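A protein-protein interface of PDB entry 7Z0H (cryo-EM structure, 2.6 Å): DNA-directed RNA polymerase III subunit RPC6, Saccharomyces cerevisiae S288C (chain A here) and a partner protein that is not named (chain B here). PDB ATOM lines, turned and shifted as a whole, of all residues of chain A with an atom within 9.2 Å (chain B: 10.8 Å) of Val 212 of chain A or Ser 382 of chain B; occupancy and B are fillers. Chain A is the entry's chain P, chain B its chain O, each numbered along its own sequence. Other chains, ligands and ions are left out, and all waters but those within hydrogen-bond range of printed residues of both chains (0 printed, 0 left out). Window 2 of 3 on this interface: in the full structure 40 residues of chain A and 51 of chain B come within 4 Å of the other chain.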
ATOM      1  N   ASN A 189      34.735 -18.916  -2.307  1.00  0.00           N
ATOM      2  CA  ASN A 189      33.408 -19.476  -2.530  1.00  0.00           C
ATOM      3  C   ASN A 189      33.087 -20.563  -1.514  1.00  0.00           C
ATOM      4  O   ASN A 189      31.934 -20.712  -1.093  1.00  0.00           O
ATOM      5  CB  ASN A 189      33.316 -20.031  -3.952  1.00  0.00           C
ATOM      6  CG  ASN A 189      31.919 -19.939  -4.528  1.00  0.00           C
ATOM      7  OD1 ASN A 189      31.272 -18.893  -4.459  1.00  0.00           O
ATOM      8  ND2 ASN A 189      31.447 -21.035  -5.108  1.00  0.00           N
ATOM      9  N   THR A 190      34.097 -21.336  -1.109  1.00  0.00           N
ATOM     10  CA  THR A 190      33.854 -22.482  -0.239  1.00  0.00           C
ATOM     11  C   THR A 190      33.547 -22.044   1.189  1.00  0.00           C
ATOM     12  O   THR A 190      32.629 -22.572   1.827  1.00  0.00           O
ATOM     13  CB  THR A 190      35.063 -23.420  -0.266  1.00  0.00           C
ATOM     14  OG1 THR A 190      35.250 -23.922  -1.596  1.00  0.00           O
ATOM     15  CG2 THR A 190      34.857 -24.585   0.681  1.00  0.00           C
ATOM     16  N   PRO A 192      32.356 -19.683   4.447  1.00  0.00           N
ATOM     17  CA  PRO A 192      31.231 -18.756   4.664  1.00  0.00           C
ATOM     18  C   PRO A 192      31.584 -17.302   4.405  1.00  0.00           C
ATOM     19  O   PRO A 192      30.771 -16.563   3.837  1.00  0.00           O
ATOM     20  CB  PRO A 192      30.867 -18.995   6.135  1.00  0.00           C
ATOM     21  CG  PRO A 192      31.310 -20.388   6.410  1.00  0.00           C
ATOM     22  CD  PRO A 192      32.544 -20.605   5.581  1.00  0.00           C
ATOM     23  N   VAL A 206      34.429 -19.496  11.276  1.00  0.00           N
ATOM     24  CA  VAL A 206      33.186 -20.253  11.245  1.00  0.00           C
ATOM     25  C   VAL A 206      33.212 -21.208  10.057  1.00  0.00           C
ATOM     26  O   VAL A 206      33.873 -20.965   9.045  1.00  0.00           O
ATOM     27  CB  VAL A 206      31.942 -19.339  11.175  1.00  0.00           C
ATOM     28  CG1 VAL A 206      31.836 -18.495  12.437  1.00  0.00           C
ATOM     29  CG2 VAL A 206      31.996 -18.455   9.940  1.00  0.00           C
ATOM     30  N   PHE A 207      32.478 -22.310  10.199  1.00  0.00           N
ATOM     31  CA  PHE A 207      32.412 -23.346   9.180  1.00  0.00           C
ATOM     32  C   PHE A 207      30.960 -23.648   8.839  1.00  0.00           C
ATOM     33  O   PHE A 207      30.048 -23.428   9.640  1.00  0.00           O
ATOM     34  CB  PHE A 207      33.117 -24.634   9.630  1.00  0.00           C
ATOM     35  CG  PHE A 207      34.553 -24.438  10.016  1.00  0.00           C
ATOM     36  CD1 PHE A 207      35.446 -23.852   9.135  1.00  0.00           C
ATOM     37  CD2 PHE A 207      35.013 -24.844  11.259  1.00  0.00           C
ATOM     38  CE1 PHE A 207      36.770 -23.671   9.486  1.00  0.00           C
ATOM     39  CE2 PHE A 207      36.335 -24.666  11.615  1.00  0.00           C
ATOM     40  CZ  PHE A 207      37.215 -24.079  10.728  1.00  0.00           C
ATOM     41  N   TYR A 208      30.761 -24.158   7.626  1.00  0.00           N
ATOM     42  CA  TYR A 208      29.425 -24.485   7.150  1.00  0.00           C
ATOM     43  C   TYR A 208      28.909 -25.772   7.785  1.00  0.00           C
ATOM     44  O   TYR A 208      29.678 -26.643   8.203  1.00  0.00           O
ATOM     45  CB  TYR A 208      29.423 -24.628   5.628  1.00  0.00           C
ATOM     46  CG  TYR A 208      29.211 -23.327   4.891  1.00  0.00           C
ATOM     47  CD1 TYR A 208      28.312 -22.380   5.361  1.00  0.00           C
ATOM     48  CD2 TYR A 208      29.904 -23.049   3.720  1.00  0.00           C
ATOM     49  CE1 TYR A 208      28.113 -21.190   4.690  1.00  0.00           C
ATOM     50  CE2 TYR A 208      29.711 -21.862   3.040  1.00  0.00           C
ATOM     51  CZ  TYR A 208      28.812 -20.937   3.529  1.00  0.00           C
ATOM     52  OH  TYR A 208      28.616 -19.752   2.857  1.00  0.00           O
ATOM     53  N   ALA A 209      27.584 -25.882   7.854  1.00  0.00           N
ATOM     54  CA  ALA A 209      26.941 -27.105   8.295  1.00  0.00           C
ATOM     55  C   ALA A 209      27.114 -28.194   7.235  1.00  0.00           C
ATOM     56  O   ALA A 209      27.355 -27.896   6.063  1.00  0.00           O
ATOM     57  CB  ALA A 209      25.461 -26.850   8.572  1.00  0.00           C
ATOM     58  N   PRO A 210      27.012 -29.471   7.628  1.00  0.00           N
ATOM     59  CA  PRO A 210      27.268 -30.548   6.652  1.00  0.00           C
ATOM     60  C   PRO A 210      26.322 -30.543   5.463  1.00  0.00           C
ATOM     61  O   PRO A 210      26.775 -30.679   4.319  1.00  0.00           O
ATOM     62  CB  PRO A 210      27.104 -31.827   7.490  1.00  0.00           C
ATOM     63  CG  PRO A 210      26.314 -31.411   8.687  1.00  0.00           C
ATOM     64  CD  PRO A 210      26.718 -30.004   8.970  1.00  0.00           C
ATOM     65  N   ASN A 211      25.020 -30.380   5.696  1.00  0.00           N
ATOM     66  CA  ASN A 211      24.032 -30.508   4.632  1.00  0.00           C
ATOM     67  C   ASN A 211      24.083 -29.370   3.619  1.00  0.00           C
ATOM     68  O   ASN A 211      23.465 -29.487   2.554  1.00  0.00           O
ATOM     69  CB  ASN A 211      22.627 -30.604   5.230  1.00  0.00           C
ATOM     70  CG  ASN A 211      22.375 -29.556   6.297  1.00  0.00           C
ATOM     71  OD1 ASN A 211      23.173 -28.638   6.482  1.00  0.00           O
ATOM     72  ND2 ASN A 211      21.261 -29.692   7.008  1.00  0.00           N
ATOM     73  N   VAL A 212      24.793 -28.281   3.916  1.00  0.00           N
ATOM     74  CA  VAL A 212      24.925 -27.190   2.959  1.00  0.00           C
ATOM     75  C   VAL A 212      25.799 -27.635   1.794  1.00  0.00           C
ATOM     76  O   VAL A 212      26.727 -28.439   1.960  1.00  0.00           O
ATOM     77  CB  VAL A 212      25.506 -25.941   3.645  1.00  0.00           C
ATOM     78  CG1 VAL A 212      25.207 -24.693   2.823  1.00  0.00           C
ATOM     79  CG2 VAL A 212      24.955 -25.806   5.055  1.00  0.00           C
ATOM     80  N   LYS A 213      25.500 -27.117   0.602  1.00  0.00           N
ATOM     81  CA  LYS A 213      26.281 -27.430  -0.595  1.00  0.00           C
ATOM     82  C   LYS A 213      27.421 -26.421  -0.711  1.00  0.00           C
ATOM     83  O   LYS A 213      27.400 -25.490  -1.520  1.00  0.00           O
ATOM     84  CB  LYS A 213      25.396 -27.429  -1.835  1.00  0.00           C
ATOM     85  CG  LYS A 213      24.348 -28.527  -1.848  1.00  0.00           C
ATOM     86  CD  LYS A 213      23.670 -28.632  -3.206  1.00  0.00           C
ATOM     87  CE  LYS A 213      22.889 -27.374  -3.543  1.00  0.00           C
ATOM     88  NZ  LYS A 213      22.104 -27.542  -4.798  1.00  0.00           N
ATOM     89  N   ASN A 214      28.440 -26.617   0.128  1.00  0.00           N
ATOM     90  CA  ASN A 214      29.626 -25.772   0.065  1.00  0.00           C
ATOM     91  C   ASN A 214      30.465 -26.046  -1.174  1.00  0.00           C
ATOM     92  O   ASN A 214      31.285 -25.202  -1.552  1.00  0.00           O
ATOM     93  CB  ASN A 214      30.480 -25.963   1.320  1.00  0.00           C
ATOM     94  CG  ASN A 214      30.847 -27.416   1.561  1.00  0.00           C
ATOM     95  OD1 ASN A 214      30.340 -28.316   0.893  1.00  0.00           O
ATOM     96  ND2 ASN A 214      31.738 -27.649   2.518  1.00  0.00           N
ATOM     97  N   TYR A 215      30.280 -27.199  -1.812  1.00  0.00           N
ATOM     98  CA  TYR A 215      31.079 -27.546  -2.976  1.00  0.00           C
ATOM     99  C   TYR A 215      30.691 -26.698  -4.181  1.00  0.00           C
ATOM    100  O   TYR A 215      29.552 -26.241  -4.313  1.00  0.00           O
ATOM    101  CB  TYR A 215      30.926 -29.032  -3.309  1.00  0.00           C
ATOM    102  CG  TYR A 215      29.516 -29.477  -3.643  1.00  0.00           C
ATOM    103  CD1 TYR A 215      29.013 -29.356  -4.933  1.00  0.00           C
ATOM    104  CD2 TYR A 215      28.700 -30.045  -2.674  1.00  0.00           C
ATOM    105  CE1 TYR A 215      27.731 -29.770  -5.244  1.00  0.00           C
ATOM    106  CE2 TYR A 215      27.416 -30.463  -2.975  1.00  0.00           C
ATOM    107  CZ  TYR A 215      26.937 -30.323  -4.262  1.00  0.00           C
ATOM    108  OH  TYR A 215      25.663 -30.738  -4.568  1.00  0.00           O
ATOM    109  N   SER A 216      31.661 -26.489  -5.066  1.00  0.00           N
ATOM    110  CA  SER A 216      31.458 -25.775  -6.317  1.00  0.00           C
ATOM    111  C   SER A 216      31.449 -26.776  -7.464  1.00  0.00           C
ATOM    112  O   SER A 216      32.203 -27.753  -7.444  1.00  0.00           O
ATOM    113  CB  SER A 216      32.552 -24.726  -6.536  1.00  0.00           C
ATOM    114  OG  SER A 216      32.660 -24.380  -7.906  1.00  0.00           O
ATOM    115  N   ARG A 262      37.647 -28.495  -2.514  1.00  0.00           N
ATOM    116  CA  ARG A 262      37.677 -27.833  -1.216  1.00  0.00           C
ATOM    117  C   ARG A 262      39.122 -27.646  -0.772  1.00  0.00           C
ATOM    118  O   ARG A 262      39.984 -28.484  -1.053  1.00  0.00           O
ATOM    119  CB  ARG A 262      36.905 -28.633  -0.157  1.00  0.00           C
ATOM    120  CG  ARG A 262      35.394 -28.459  -0.205  1.00  0.00           C
ATOM    121  CD  ARG A 262      34.771 -28.616   1.172  1.00  0.00           C
ATOM    122  NE  ARG A 262      35.135 -27.521   2.064  1.00  0.00           N
ATOM    123  CZ  ARG A 262      36.064 -27.598   3.007  1.00  0.00           C
ATOM    124  NH1 ARG A 262      36.739 -28.716   3.222  1.00  0.00           N
ATOM    125  NH2 ARG A 262      36.319 -26.529   3.755  1.00  0.00           N
ATOM    126  N   LEU B 376      31.094 -24.559  21.372  1.00  0.00           N
ATOM    127  CA  LEU B 376      30.407 -25.223  20.267  1.00  0.00           C
ATOM    128  C   LEU B 376      29.187 -24.454  19.780  1.00  0.00           C
ATOM    129  O   LEU B 376      28.220 -25.070  19.316  1.00  0.00           O
ATOM    130  CB  LEU B 376      29.979 -26.648  20.636  1.00  0.00           C
ATOM    131  CG  LEU B 376      31.062 -27.640  21.041  1.00  0.00           C
ATOM    132  CD1 LEU B 376      30.849 -28.031  22.495  1.00  0.00           C
ATOM    133  CD2 LEU B 376      31.085 -28.858  20.135  1.00  0.00           C
ATOM    134  N   ARG B 377      29.196 -23.125  19.875  1.00  0.00           N
ATOM    135  CA  ARG B 377      28.006 -22.352  19.529  1.00  0.00           C
ATOM    136  C   ARG B 377      28.175 -21.640  18.190  1.00  0.00           C
ATOM    137  O   ARG B 377      27.338 -21.776  17.292  1.00  0.00           O
ATOM    138  CB  ARG B 377      27.695 -21.356  20.649  1.00  0.00           C
ATOM    139  CG  ARG B 377      27.395 -22.023  21.987  1.00  0.00           C
ATOM    140  CD  ARG B 377      27.043 -21.003  23.058  1.00  0.00           C
ATOM    141  NE  ARG B 377      26.575 -21.629  24.289  1.00  0.00           N
ATOM    142  CZ  ARG B 377      27.338 -21.867  25.347  1.00  0.00           C
ATOM    143  NH1 ARG B 377      28.629 -21.580  25.347  1.00  0.00           N
ATOM    144  NH2 ARG B 377      26.791 -22.401  26.436  1.00  0.00           N
ATOM    145  N   GLY B 378      29.257 -20.882  18.039  1.00  0.00           N
ATOM    146  CA  GLY B 378      29.535 -20.206  16.787  1.00  0.00           C
ATOM    147  C   GLY B 378      30.296 -21.083  15.814  1.00  0.00           C
ATOM    148  O   GLY B 378      30.851 -20.598  14.825  1.00  0.00           O
ATOM    149  N   SER B 379      30.332 -22.386  16.098  1.00  0.00           N
ATOM    150  CA  SER B 379      31.069 -23.329  15.269  1.00  0.00           C
ATOM    151  C   SER B 379      30.360 -23.665  13.963  1.00  0.00           C
ATOM    152  O   SER B 379      31.023 -24.080  13.007  1.00  0.00           O
ATOM    153  CB  SER B 379      31.330 -24.619  16.051  1.00  0.00           C
ATOM    154  OG  SER B 379      31.718 -24.338  17.385  1.00  0.00           O
ATOM    155  N   LEU B 380      29.042 -23.500  13.898  1.00  0.00           N
ATOM    156  CA  LEU B 380      28.260 -23.920  12.744  1.00  0.00           C
ATOM    157  C   LEU B 380      27.516 -22.739  12.139  1.00  0.00           C
ATOM    158  O   LEU B 380      27.018 -21.868  12.859  1.00  0.00           O
ATOM    159  CB  LEU B 380      27.248 -25.012  13.115  1.00  0.00           C
ATOM    160  CG  LEU B 380      27.726 -26.465  13.085  1.00  0.00           C
ATOM    161  CD1 LEU B 380      28.272 -26.837  11.713  1.00  0.00           C
ATOM    162  CD2 LEU B 380      28.748 -26.721  14.169  1.00  0.00           C
ATOM    163  N   LEU B 381      27.445 -22.723  10.811  1.00  0.00           N
ATOM    164  CA  LEU B 381      26.613 -21.788  10.062  1.00  0.00           C
ATOM    165  C   LEU B 381      25.689 -22.618   9.177  1.00  0.00           C
ATOM    166  O   LEU B 381      26.112 -23.126   8.133  1.00  0.00           O
ATOM    167  CB  LEU B 381      27.467 -20.827   9.240  1.00  0.00           C
ATOM    168  CG  LEU B 381      26.713 -19.685   8.559  1.00  0.00           C
ATOM    169  CD1 LEU B 381      26.188 -18.692   9.587  1.00  0.00           C
ATOM    170  CD2 LEU B 381      27.587 -18.987   7.532  1.00  0.00           C
ATOM    171  N   SER B 382      24.429 -22.757   9.601  1.00  0.00           N
ATOM    172  CA  SER B 382      23.525 -23.709   8.961  1.00  0.00           C
ATOM    173  C   SER B 382      23.179 -23.314   7.529  1.00  0.00           C
ATOM    174  O   SER B 382      22.732 -24.161   6.749  1.00  0.00           O
ATOM    175  CB  SER B 382      22.248 -23.857   9.789  1.00  0.00           C
ATOM    176  OG  SER B 382      22.548 -24.097  11.153  1.00  0.00           O
ATOM    177  N   ARG B 383      23.370 -22.048   7.163  1.00  0.00           N
ATOM    178  CA  ARG B 383      23.046 -21.582   5.822  1.00  0.00           C
ATOM    179  C   ARG B 383      24.092 -20.580   5.360  1.00  0.00           C
ATOM    180  O   ARG B 383      24.705 -19.881   6.170  1.00  0.00           O
ATOM    181  CB  ARG B 383      21.650 -20.947   5.769  1.00  0.00           C
ATOM    182  CG  ARG B 383      21.483 -19.744   6.682  1.00  0.00           C
ATOM    183  CD  ARG B 383      20.078 -19.174   6.593  1.00  0.00           C
ATOM    184  NE  ARG B 383      19.068 -20.128   7.035  1.00  0.00           N
ATOM    185  CZ  ARG B 383      18.720 -20.318   8.299  1.00  0.00           C
ATOM    186  NH1 ARG B 383      19.288 -19.639   9.282  1.00  0.00           N
ATOM    187  NH2 ARG B 383      17.776 -21.210   8.586  1.00  0.00           N
ATOM    188  N   LYS B 384      24.284 -20.514   4.045  1.00  0.00           N
ATOM    189  CA  LYS B 384      25.255 -19.603   3.442  1.00  0.00           C
ATOM    190  C   LYS B 384      24.976 -18.149   3.810  1.00  0.00           C
ATOM    191  O   LYS B 384      25.898 -17.339   3.920  1.00  0.00           O
ATOM    192  CB  LYS B 384      25.261 -19.760   1.919  1.00  0.00           C
ATOM    193  CG  LYS B 384      25.795 -21.095   1.426  1.00  0.00           C
ATOM    194  CD  LYS B 384      25.632 -21.231  -0.082  1.00  0.00           C
ATOM    195  CE  LYS B 384      26.612 -20.344  -0.834  1.00  0.00           C
ATOM    196  NZ  LYS B 384      28.026 -20.768  -0.626  1.00  0.00           N
ATOM    197  N   SER B 449      25.253 -28.876  23.285  1.00  0.00           N
ATOM    198  CA  SER B 449      24.041 -29.357  22.638  1.00  0.00           C
ATOM    199  C   SER B 449      24.343 -30.598  21.807  1.00  0.00           C
ATOM    200  O   SER B 449      25.150 -30.552  20.875  1.00  0.00           O
ATOM    201  CB  SER B 449      23.442 -28.262  21.757  1.00  0.00           C
ATOM    202  OG  SER B 449      24.345 -27.884  20.733  1.00  0.00           O
ATOM    203  N   SER B 451      22.889 -31.943  19.513  1.00  0.00           N
ATOM    204  CA  SER B 451      22.686 -31.780  18.078  1.00  0.00           C
ATOM    205  C   SER B 451      23.970 -31.335  17.388  1.00  0.00           C
ATOM    206  O   SER B 451      24.344 -31.871  16.338  1.00  0.00           O
ATOM    207  CB  SER B 451      21.560 -30.778  17.821  1.00  0.00           C
ATOM    208  OG  SER B 451      21.565 -30.337  16.474  1.00  0.00           O
ATOM    209  N   LEU B 452      24.666 -30.358  17.973  1.00  0.00           N
ATOM    210  CA  LEU B 452      25.786 -29.718  17.289  1.00  0.00           C
ATOM    211  C   LEU B 452      27.033 -30.598  17.267  1.00  0.00           C
ATOM    212  O   LEU B 452      27.756 -30.621  16.265  1.00  0.00           O
ATOM    213  CB  LEU B 452      26.088 -28.368  17.938  1.00  0.00           C
ATOM    214  CG  LEU B 452      25.214 -27.227  17.415  1.00  0.00           C
ATOM    215  CD1 LEU B 452      25.371 -25.975  18.261  1.00  0.00           C
ATOM    216  CD2 LEU B 452      25.523 -26.938  15.955  1.00  0.00           C
ATOM    217  N   SER B 455      26.634 -32.772  14.650  1.00  0.00           N
ATOM    218  CA  SER B 455      26.920 -32.116  13.374  1.00  0.00           C
ATOM    219  C   SER B 455      28.411 -32.147  13.045  1.00  0.00           C
ATOM    220  O   SER B 455      28.794 -32.413  11.898  1.00  0.00           O
ATOM    221  CB  SER B 455      26.403 -30.677  13.396  1.00  0.00           C
ATOM    222  OG  SER B 455      27.067 -29.885  12.428  1.00  0.00           O
ATOM    223  N   HIS B 456      29.269 -31.862  14.032  1.00  0.00           N
ATOM    224  CA  HIS B 456      30.706 -32.048  13.836  1.00  0.00           C
ATOM    225  C   HIS B 456      31.014 -33.481  13.436  1.00  0.00           C
ATOM    226  O   HIS B 456      31.909 -33.738  12.626  1.00  0.00           O
ATOM    227  CB  HIS B 456      31.478 -31.702  15.110  1.00  0.00           C
ATOM    228  CG  HIS B 456      31.430 -30.256  15.484  1.00  0.00           C
ATOM    229  ND1 HIS B 456      31.847 -29.798  16.715  1.00  0.00           N
ATOM    230  CD2 HIS B 456      31.041 -29.163  14.788  1.00  0.00           C
ATOM    231  CE1 HIS B 456      31.703 -28.487  16.767  1.00  0.00           C
ATOM    232  NE2 HIS B 456      31.218 -28.077  15.610  1.00  0.00           N
ATOM    233  N   LYS B 458      29.016 -35.619  11.829  1.00  0.00           N
ATOM    234  CA  LYS B 458      28.615 -35.785  10.433  1.00  0.00           C
ATOM    235  C   LYS B 458      29.625 -35.157   9.479  1.00  0.00           C
ATOM    236  O   LYS B 458      29.928 -35.737   8.433  1.00  0.00           O
ATOM    237  CB  LYS B 458      27.225 -35.192  10.181  1.00  0.00           C
ATOM    238  CG  LYS B 458      26.144 -35.634  11.148  1.00  0.00           C
ATOM    239  CD  LYS B 458      24.743 -35.402  10.589  1.00  0.00           C
ATOM    240  CE  LYS B 458      23.915 -36.680  10.629  1.00  0.00           C
ATOM    241  NZ  LYS B 458      22.458 -36.432  10.803  1.00  0.00           N
ATOM    242  N   ILE B 459      30.141 -33.967   9.802  1.00  0.00           N
ATOM    243  CA  ILE B 459      31.121 -33.361   8.897  1.00  0.00           C
ATOM    244  C   ILE B 459      32.420 -34.158   8.912  1.00  0.00           C
ATOM    245  O   ILE B 459      33.104 -34.260   7.886  1.00  0.00           O
ATOM    246  CB  ILE B 459      31.367 -31.869   9.216  1.00  0.00           C
ATOM    247  CG1 ILE B 459      32.180 -31.684  10.497  1.00  0.00           C
ATOM    248  CG2 ILE B 459      30.060 -31.114   9.306  1.00  0.00           C
ATOM    249  CD1 ILE B 459      32.480 -30.240  10.831  1.00  0.00           C
ATOM    250  N   SER B 462      31.707 -37.084   6.646  1.00  0.00           N
ATOM    251  CA  SER B 462      31.561 -36.621   5.272  1.00  0.00           C
ATOM    252  C   SER B 462      32.831 -35.994   4.718  1.00  0.00           C
ATOM    253  O   SER B 462      32.874 -35.670   3.525  1.00  0.00           O
ATOM    254  CB  SER B 462      30.412 -35.610   5.175  1.00  0.00           C
ATOM    255  OG  SER B 462      30.533 -34.810   4.011  1.00  0.00           O
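The backbone NH (N) of Leu 381 of chain B is in hydrogen-bond range of the backbone carbonyl oxygen (O) of Phe 207 of chain A, 2.9 Å away.
The backbone carbonyl oxygen of Leu 381 of chain B lies within hydrogen-bond range of the backbone NH of Ala 209 of chain A, 3.1 Å away.
Among the printed residues, pairs that only touch across the chains: Asn 189 of chain A with Lys 384 of chain B (3.9 Å), Pro 192 of chain A with Leu 381 of chain B (3.6 Å), Val 206 of chain A with Gly 378 of chain B (3.3 Å), Phe 207 of chain A with Ser 379 of chain B (3.6 Å), Phe 207 of chain A with Leu 380 of chain B (3.6 Å), Tyr 208 of chain A with Leu 380 of chain B (3.8 Å), Tyr 208 of chain A with Leu 381 of chain B (3.6 Å), Tyr 208 of chain A with Arg 383 of chain B (3.9 Å), Tyr 208 of chain A with Lys 384 of chain B (3.4 Å), Ala 209 of chain A with Leu 380 of chain B (3.7 Å), Ala 209 of chain A with Ser 382 of chain B (3.7 Å), Pro 210 of chain A with Ser 455 of chain B (3.5 Å), Pro 210 of chain A with Ile 459 of chain B (3.5 Å), Val 212 of chain A with Ser 382 of chain B (3.2 Å) and Val 212 of chain A with Lys 384 of chain B (3.9 Å).
Of the printed residues of chain B, Pro 192 of chain A touches Leu 381 (3.6 Å).
Of chain B, only Leu 380, Leu 381, Arg 383 and Lys 384 come within 4 Å of Tyr 208 of chain A.
Ala 209 of chain A touches three residues of chain B.
Of chain B, only Ser 455 and Ile 459 come within 4 Å of Pro 210 of chain A.
No residue of chain B comes within 4 Å of Asn 211 of chain A.
Val 212 of chain A touches two residues of chain B.
Arg 262 of chain A touches none of the printed residues of chain B.
Of the printed residues of chain A, Leu 380 of chain B touches Phe 207, Tyr 208 and Ala 209.
Printed residues of chain A within 4 Å of Ser 455 of chain B: Pro 210.
Ser 462 of chain B touches none of the printed residues of chain A.
Of the 17 printed residues of chain B, 9 touch a printed residue of chain A.
Printed residues of chain B that touch a printed residue of chain A: Gly 378, Ser 379, Leu 380, Leu 381, Ser 382, Arg 383, Lys 384, Ser 455 and Ile 459.
Hydrophobic or aromatic side chains of chain A that line the printed part of chain B: Pro 192, Val 206, Tyr 208, Ala 209, Pro 210 and Val 212.
Among the printed residues, no Asp or Glu carboxylate lies within 4 Å of a Lys or Arg side-chain nitrogen of the other chain.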
